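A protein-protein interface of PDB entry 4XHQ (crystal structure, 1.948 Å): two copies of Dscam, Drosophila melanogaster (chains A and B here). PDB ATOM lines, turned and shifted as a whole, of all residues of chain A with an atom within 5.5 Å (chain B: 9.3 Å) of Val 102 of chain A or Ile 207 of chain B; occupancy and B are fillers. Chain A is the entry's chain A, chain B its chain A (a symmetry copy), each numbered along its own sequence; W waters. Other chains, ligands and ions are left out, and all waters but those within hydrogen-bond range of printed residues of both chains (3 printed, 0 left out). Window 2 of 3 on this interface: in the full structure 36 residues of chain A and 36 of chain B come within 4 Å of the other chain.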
ATOM      1  N   PHE A  16       2.051  14.571  -9.861  1.00  0.00           N
ATOM      2  CA  PHE A  16       2.046  15.785 -10.697  1.00  0.00           C
ATOM      3  C   PHE A  16       0.760  16.557 -10.493  1.00  0.00           C
ATOM      4  O   PHE A  16      -0.259  15.969 -10.102  1.00  0.00           O
ATOM      5  CB  PHE A  16       2.255  15.405 -12.186  1.00  0.00           C
ATOM      6  CG  PHE A  16       1.254  14.388 -12.698  1.00  0.00           C
ATOM      7  CD1 PHE A  16       1.426  13.026 -12.446  1.00  0.00           C
ATOM      8  CD2 PHE A  16       0.134  14.793 -13.456  1.00  0.00           C
ATOM      9  CE1 PHE A  16       0.465  12.069 -12.930  1.00  0.00           C
ATOM     10  CE2 PHE A  16      -0.790  13.869 -13.959  1.00  0.00           C
ATOM     11  CZ  PHE A  16      -0.630  12.502 -13.698  1.00  0.00           C
ATOM     12  N   SER A  17       0.785  17.893 -10.707  1.00  0.00           N
ATOM     13  CA  SER A  17      -0.473  18.655 -10.588  1.00  0.00           C
ATOM     14  C   SER A  17      -1.248  18.520 -11.891  1.00  0.00           C
ATOM     15  O   SER A  17      -0.651  18.205 -12.920  1.00  0.00           O
ATOM     16  CB  SER A  17      -0.249  20.160 -10.329  1.00  0.00           C
ATOM     17  OG  SER A  17       0.269  20.702 -11.521  1.00  0.00           O
ATOM     18  N   ASN A  18      -2.555  18.729 -11.812  1.00  0.00           N
ATOM     19  CA  ASN A  18      -3.399  18.731 -13.018  1.00  0.00           C
ATOM     20  C   ASN A  18      -2.892  19.706 -14.070  1.00  0.00           C
ATOM     21  O   ASN A  18      -3.170  19.493 -15.247  1.00  0.00           O
ATOM     22  CB  ASN A  18      -4.832  19.050 -12.653  1.00  0.00           C
ATOM     23  CG  ASN A  18      -4.966  20.494 -12.116  1.00  0.00           C
ATOM     24  OD1 ASN A  18      -4.387  20.854 -11.070  1.00  0.00           O
ATOM     25  ND2 ASN A  18      -5.698  21.331 -12.857  1.00  0.00           N
ATOM     26  N   PHE A  66      -5.309  18.790 -17.191  1.00  0.00           N
ATOM     27  CA  PHE A  66      -6.752  18.647 -17.200  1.00  0.00           C
ATOM     28  C   PHE A  66      -7.335  19.568 -16.155  1.00  0.00           C
ATOM     29  O   PHE A  66      -6.638  19.981 -15.238  1.00  0.00           O
ATOM     30  CB  PHE A  66      -7.202  17.192 -16.915  1.00  0.00           C
ATOM     31  CG  PHE A  66      -6.802  16.681 -15.504  1.00  0.00           C
ATOM     32  CD1 PHE A  66      -5.518  16.226 -15.274  1.00  0.00           C
ATOM     33  CD2 PHE A  66      -7.711  16.703 -14.450  1.00  0.00           C
ATOM     34  CE1 PHE A  66      -5.114  15.761 -13.988  1.00  0.00           C
ATOM     35  CE2 PHE A  66      -7.321  16.246 -13.149  1.00  0.00           C
ATOM     36  CZ  PHE A  66      -6.018  15.797 -12.958  1.00  0.00           C
ATOM     37  N   ALA A  68      -9.930  20.636 -13.121  1.00  0.00           N
ATOM     38  CA  ALA A  68     -10.329  20.032 -11.869  1.00  0.00           C
ATOM     39  C   ALA A  68     -11.568  19.214 -12.014  1.00  0.00           C
ATOM     40  O   ALA A  68     -11.689  18.126 -11.462  1.00  0.00           O
ATOM     41  CB  ALA A  68     -10.539  21.152 -10.789  1.00  0.00           C
ATOM     42  N   TYR A  71     -11.171  15.449 -13.192  1.00  0.00           N
ATOM     43  CA  TYR A  71     -10.463  14.447 -12.389  1.00  0.00           C
ATOM     44  C   TYR A  71     -11.210  13.087 -12.403  1.00  0.00           C
ATOM     45  O   TYR A  71     -12.430  12.985 -12.144  1.00  0.00           O
ATOM     46  CB  TYR A  71     -10.297  14.945 -10.930  1.00  0.00           C
ATOM     47  CG  TYR A  71      -9.556  13.959 -10.053  1.00  0.00           C
ATOM     48  CD1 TYR A  71     -10.251  12.991  -9.328  1.00  0.00           C
ATOM     49  CD2 TYR A  71      -8.171  13.995  -9.969  1.00  0.00           C
ATOM     50  CE1 TYR A  71      -9.549  12.079  -8.494  1.00  0.00           C
ATOM     51  CE2 TYR A  71      -7.477  13.122  -9.135  1.00  0.00           C
ATOM     52  CZ  TYR A  71      -8.180  12.170  -8.433  1.00  0.00           C
ATOM     53  OH  TYR A  71      -7.441  11.297  -7.682  1.00  0.00           O
ATOM     54  N   ALA A 100      -2.087  12.129  -9.765  1.00  0.00           N
ATOM     55  CA  ALA A 100      -2.344  13.484 -10.289  1.00  0.00           C
ATOM     56  C   ALA A 100      -3.088  14.234  -9.184  1.00  0.00           C
ATOM     57  O   ALA A 100      -4.093  13.757  -8.708  1.00  0.00           O
ATOM     58  CB  ALA A 100      -3.178  13.465 -11.534  1.00  0.00           C
ATOM     59  N   VAL A 101      -2.576  15.392  -8.769  1.00  0.00           N
ATOM     60  CA  VAL A 101      -3.257  16.130  -7.676  1.00  0.00           C
ATOM     61  C   VAL A 101      -3.732  17.484  -8.239  1.00  0.00           C
ATOM     62  O   VAL A 101      -2.909  18.250  -8.771  1.00  0.00           O
ATOM     63  CB  VAL A 101      -2.250  16.371  -6.490  1.00  0.00           C
ATOM     64  CG1 VAL A 101      -2.951  17.128  -5.343  1.00  0.00           C
ATOM     65  CG2 VAL A 101      -1.643  15.005  -6.015  1.00  0.00           C
ATOM     66  N   VAL A 102      -5.013  17.758  -8.112  1.00  0.00           N
ATOM     67  CA  VAL A 102      -5.557  19.019  -8.600  1.00  0.00           C
ATOM     68  C   VAL A 102      -5.012  20.157  -7.672  1.00  0.00           C
ATOM     69  O   VAL A 102      -5.029  20.006  -6.445  1.00  0.00           O
ATOM     70  CB  VAL A 102      -7.060  19.016  -8.549  1.00  0.00           C
ATOM     71  CG1 VAL A 102      -7.578  20.401  -8.941  1.00  0.00           C
ATOM     72  CG2 VAL A 102      -7.678  17.884  -9.444  1.00  0.00           C
ATOM     73  N   ALA A 103      -4.439  21.190  -8.254  1.00  0.00           N
ATOM     74  CA  ALA A 103      -3.947  22.343  -7.474  1.00  0.00           C
ATOM     75  C   ALA A 103      -5.066  22.872  -6.607  1.00  0.00           C
ATOM     76  O   ALA A 103      -6.188  23.124  -7.061  1.00  0.00           O
ATOM     77  CB  ALA A 103      -3.382  23.410  -8.395  1.00  0.00           C
ATOM     78  N   GLN A 104      -4.794  22.979  -5.312  1.00  0.00           N
ATOM     79  CA  GLN A 104      -5.831  23.323  -4.369  1.00  0.00           C
ATOM     80  C   GLN A 104      -5.223  24.034  -3.162  1.00  0.00           C
ATOM     81  O   GLN A 104      -4.117  23.697  -2.697  1.00  0.00           O
ATOM     82  CB  GLN A 104      -6.589  22.076  -3.907  1.00  0.00           C
ATOM     83  CG  GLN A 104      -7.678  22.327  -2.852  1.00  0.00           C
ATOM     84  CD  GLN A 104      -8.495  21.068  -2.614  1.00  0.00           C
ATOM     85  OE1 GLN A 104      -8.017  19.947  -2.883  1.00  0.00           O
ATOM     86  NE2 GLN A 104      -9.762  21.245  -2.215  1.00  0.00           N
ATOM     87  N   ILE B 116     -11.128  16.554   5.661  1.00  0.00           N
ATOM     88  CA  ILE B 116     -11.718  16.447   4.315  1.00  0.00           C
ATOM     89  C   ILE B 116     -13.208  16.255   4.477  1.00  0.00           C
ATOM     90  O   ILE B 116     -13.654  15.440   5.277  1.00  0.00           O
ATOM     91  CB  ILE B 116     -11.114  15.289   3.518  1.00  0.00           C
ATOM     92  CG1 ILE B 116      -9.639  15.542   3.328  1.00  0.00           C
ATOM     93  CG2 ILE B 116     -11.901  15.110   2.183  1.00  0.00           C
ATOM     94  CD1 ILE B 116      -8.817  14.323   2.780  1.00  0.00           C
ATOM     95  N   ARG B 117     -14.017  17.028   3.738  1.00  0.00           N
ATOM     96  CA  ARG B 117     -15.441  16.846   3.853  1.00  0.00           C
ATOM     97  C   ARG B 117     -15.887  15.362   3.758  1.00  0.00           C
ATOM     98  O   ARG B 117     -15.363  14.605   2.918  1.00  0.00           O
ATOM     99  CB  ARG B 117     -16.162  17.669   2.745  1.00  0.00           C
ATOM    100  CG  ARG B 117     -17.655  17.434   2.709  1.00  0.00           C
ATOM    101  CD  ARG B 117     -18.205  17.875   1.350  1.00  0.00           C
ATOM    102  NE  ARG B 117     -19.653  18.024   1.387  1.00  0.00           N
ATOM    103  CZ  ARG B 117     -20.331  18.852   0.599  1.00  0.00           C
ATOM    104  NH1 ARG B 117     -19.682  19.602  -0.292  1.00  0.00           N
ATOM    105  NH2 ARG B 117     -21.652  18.930   0.702  1.00  0.00           N
ATOM    106  N   THR B 204     -11.786  20.869   3.911  1.00  0.00           N
ATOM    107  CA  THR B 204     -11.247  20.872   2.573  1.00  0.00           C
ATOM    108  C   THR B 204     -12.248  20.113   1.658  1.00  0.00           C
ATOM    109  O   THR B 204     -12.690  18.997   1.967  1.00  0.00           O
ATOM    110  CB  THR B 204      -9.867  20.240   2.519  1.00  0.00           C
ATOM    111  OG1 THR B 204      -8.878  21.168   3.001  1.00  0.00           O
ATOM    112  CG2 THR B 204      -9.502  19.878   1.076  1.00  0.00           C
ATOM    113  N   GLU B 205     -12.619  20.719   0.539  1.00  0.00           N
ATOM    114  CA  GLU B 205     -13.461  20.004  -0.449  1.00  0.00           C
ATOM    115  C   GLU B 205     -12.667  18.907  -1.127  1.00  0.00           C
ATOM    116  O   GLU B 205     -11.532  19.127  -1.561  1.00  0.00           O
ATOM    117  CB  GLU B 205     -14.012  20.966  -1.501  1.00  0.00           C
ATOM    118  CG  GLU B 205     -15.197  21.756  -0.977  1.00  0.00           C
ATOM    119  CD  GLU B 205     -16.310  20.844  -0.462  1.00  0.00           C
ATOM    120  OE1 GLU B 205     -16.664  19.858  -1.171  1.00  0.00           O
ATOM    121  OE2 GLU B 205     -16.816  21.124   0.657  1.00  0.00           O
ATOM    122  N   PRO B 206     -13.249  17.717  -1.230  1.00  0.00           N
ATOM    123  CA  PRO B 206     -12.443  16.698  -1.921  1.00  0.00           C
ATOM    124  C   PRO B 206     -12.542  16.840  -3.456  1.00  0.00           C
ATOM    125  O   PRO B 206     -13.576  16.595  -4.051  1.00  0.00           O
ATOM    126  CB  PRO B 206     -13.041  15.367  -1.434  1.00  0.00           C
ATOM    127  CG  PRO B 206     -14.442  15.673  -1.029  1.00  0.00           C
ATOM    128  CD  PRO B 206     -14.465  17.173  -0.603  1.00  0.00           C
ATOM    129  N   ILE B 207     -11.446  17.275  -4.044  1.00  0.00           N
ATOM    130  CA  ILE B 207     -11.306  17.489  -5.464  1.00  0.00           C
ATOM    131  C   ILE B 207     -10.447  16.349  -6.017  1.00  0.00           C
ATOM    132  O   ILE B 207     -10.692  15.864  -7.095  1.00  0.00           O
ATOM    133  CB  ILE B 207     -10.646  18.877  -5.736  1.00  0.00           C
ATOM    134  CG1 ILE B 207     -11.499  20.006  -5.161  1.00  0.00           C
ATOM    135  CG2 ILE B 207     -10.487  19.131  -7.190  1.00  0.00           C
ATOM    136  CD1 ILE B 207     -12.866  20.065  -5.781  1.00  0.00           C
ATOM    137  N   SER B 208      -9.422  15.916  -5.275  1.00  0.00           N
ATOM    138  CA  SER B 208      -8.605  14.742  -5.672  1.00  0.00           C
ATOM    139  C   SER B 208      -8.907  13.620  -4.707  1.00  0.00           C
ATOM    140  O   SER B 208      -9.261  13.895  -3.584  1.00  0.00           O
ATOM    141  CB  SER B 208      -7.095  15.008  -5.619  1.00  0.00           C
ATOM    142  OG  SER B 208      -6.722  16.156  -6.311  1.00  0.00           O
ATOM    143  N   SER B 209      -8.803  12.364  -5.148  1.00  0.00           N
ATOM    144  CA  SER B 209      -8.865  11.219  -4.243  1.00  0.00           C
ATOM    145  C   SER B 209      -7.549  11.123  -3.524  1.00  0.00           C
ATOM    146  O   SER B 209      -6.529  11.548  -4.054  1.00  0.00           O
ATOM    147  CB  SER B 209      -9.163   9.918  -5.036  1.00  0.00           C
ATOM    148  OG  SER B 209     -10.520  10.024  -5.451  1.00  0.00           O
ATOM    149  N   SER B 210      -7.552  10.554  -2.315  1.00  0.00           N
ATOM    150  CA  SER B 210      -6.274  10.257  -1.664  1.00  0.00           C
ATOM    151  C   SER B 210      -6.422   9.091  -0.674  1.00  0.00           C
ATOM    152  O   SER B 210      -7.477   8.937  -0.010  1.00  0.00           O
ATOM    153  CB  SER B 210      -5.716  11.492  -0.891  1.00  0.00           C
ATOM    154  OG  SER B 210      -6.662  11.909   0.091  1.00  0.00           O
ATOM    155  N   GLY B 238      -8.947  10.759   4.455  1.00  0.00           N
ATOM    156  CA  GLY B 238      -8.675  10.473   3.040  1.00  0.00           C
ATOM    157  C   GLY B 238      -9.937  10.720   2.232  1.00  0.00           C
ATOM    158  O   GLY B 238     -10.985  11.034   2.802  1.00  0.00           O
ATOM    159  N   PHE B 239      -9.826  10.531   0.916  1.00  0.00           N
ATOM    160  CA  PHE B 239     -11.001  10.601   0.047  1.00  0.00           C
ATOM    161  C   PHE B 239     -10.916   9.522  -1.050  1.00  0.00           C
ATOM    162  O   PHE B 239      -9.922   9.452  -1.745  1.00  0.00           O
ATOM    163  CB  PHE B 239     -11.185  11.984  -0.630  1.00  0.00           C
ATOM    164  CG  PHE B 239     -12.537  12.083  -1.297  1.00  0.00           C
ATOM    165  CD1 PHE B 239     -13.687  12.240  -0.521  1.00  0.00           C
ATOM    166  CD2 PHE B 239     -12.674  11.835  -2.647  1.00  0.00           C
ATOM    167  CE1 PHE B 239     -14.952  12.279  -1.107  1.00  0.00           C
ATOM    168  CE2 PHE B 239     -13.927  11.852  -3.239  1.00  0.00           C
ATOM    169  CZ  PHE B 239     -15.069  12.074  -2.470  1.00  0.00           C
ATOM    170  N   PRO B 240     -11.925   8.667  -1.141  1.00  0.00           N
ATOM    171  CA  PRO B 240     -13.157   8.584  -0.351  1.00  0.00           C
ATOM    172  C   PRO B 240     -12.970   8.445   1.176  1.00  0.00           C
ATOM    173  O   PRO B 240     -11.895   7.995   1.625  1.00  0.00           O
ATOM    174  CB  PRO B 240     -13.839   7.308  -0.916  1.00  0.00           C
ATOM    175  CG  PRO B 240     -13.396   7.308  -2.368  1.00  0.00           C
ATOM    176  CD  PRO B 240     -11.938   7.699  -2.274  1.00  0.00           C
HETATM  177  O   HOH W   1     -11.585  23.316  -0.274  1.00  0.00           O
HETATM  178  O   HOH W   2     -12.071  17.323  -8.983  1.00  0.00           O
HETATM  179  O   HOH W   3      -6.254  18.409  -4.711  1.00  0.00           O
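Of the 11 printed residues of chain A, 4 touch a printed residue of chain B.
Printed residues of chain A that touch a printed residue of chain B: Tyr 71, Val 101, Val 102 and Gln 104.
Of the 12 printed residues of chain B, 5 touch a printed residue of chain A.
Printed residues of chain B that touch a printed residue of chain A: Thr 204, Glu 205, Ile 207, Ser 208 and Ser 209.
Among the printed residues, 9 pairs touch across the chains.
Among the printed residues, no Asp or Glu carboxylate lies within 4 Å of a Lys or Arg side-chain nitrogen of the other chain.
NE2 of Gln 104 of chain A sits at hydrogen-bond distance from O of Glu 205 of chain B (2.8 Å).
The side-chain hydroxyl (OH) of Tyr 71 of chain A sits at hydrogen-bond distance from the backbone NH (N) of Ser 209 of chain B (3.1 Å).
N of Val 102 of chain A lies within hydrogen-bond range of OG of Ser 208 of chain B (3.0 Å).
No residue of chain B comes within 4 Å of Ala 68 of chain A.
Val 101 of chain A touches just one residue of chain B: Ser 208.
Of chain B, only Ile 207 and Ser 208 come within 4 Å of Val 102 of chain A.
Ala 103 of chain A touches none of the printed residues of chain B.
Of the printed residues of chain A, Thr 204 of chain B touches Gln 104.
Ile 207 of chain B touches three residues of chain A.
Of the printed residues of chain A, Ser 209 of chain B touches Tyr 71.
The nearest residue of chain B that does not touch Val 102 of chain A is Ser 209 of chain B (7.1 Å).
The nearest residue of chain A that does not touch Ile 207 of chain B is Ala 68 of chain A (4.1 Å).
No position is printed for both chains.
Of the 9 pairs that touch across the chains among the printed residues, none has its exchanged pair printed and touching as well.
Water W2 lies within hydrogen-bond range of the backbone carbonyl oxygen of Ala 68 of chain A (2.6 Å) and the backbone carbonyl oxygen of Ile 207 of chain B (2.8 Å).
Water W3 lies within hydrogen-bond range of the backbone carbonyl oxygen (O) of Val 102 of chain A (2.7 Å), the side-chain hydroxyl (OG) of Ser 208 of chain B (2.8 Å) and the side-chain amide oxygen (OE1) of Gln 104 of chain A (3.0 Å).
Water W1 lies within hydrogen-bond range of the backbone NH of Glu 205 of chain B (2.9 Å) and the side-chain amide nitrogen of Gln 104 of chain A (3.4 Å).
The backbone NH (N) of Arg 117 of chain B is in hydrogen-bond range of the backbone carbonyl oxygen (O) of Thr 204 of chain B (3.0 Å).
The backbone NH (N) of Val 101 of chain A lies within hydrogen-bond range of the backbone carbonyl oxygen (O) of Phe 16 of chain A (2.7 Å).
The guanidinium group (NH1) of Arg 117 of chain B is in salt-bridge range of the side-chain carboxylate (OE1) of Glu 205 of chain B (3.2 Å).
The backbone NH of Asn 18 of chain A sits at hydrogen-bond distance from the backbone carbonyl oxygen of Val 101 of chain A.
Among the printed residues, pairs that only touch across the chains: Tyr 71 of chain A with Ile 207 of chain B (3.7 Å), Tyr 71 of chain A with Ser 208 of chain B (3.8 Å), Val 101 of chain A with Ser 208 of chain B (3.7 Å), Val 102 of chain A with Ile 207 of chain B (3.6 Å), Gln 104 of chain A with Thr 204 of chain B (3.6 Å) and Gln 104 of chain A with Ile 207 of chain B (3.6 Å).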
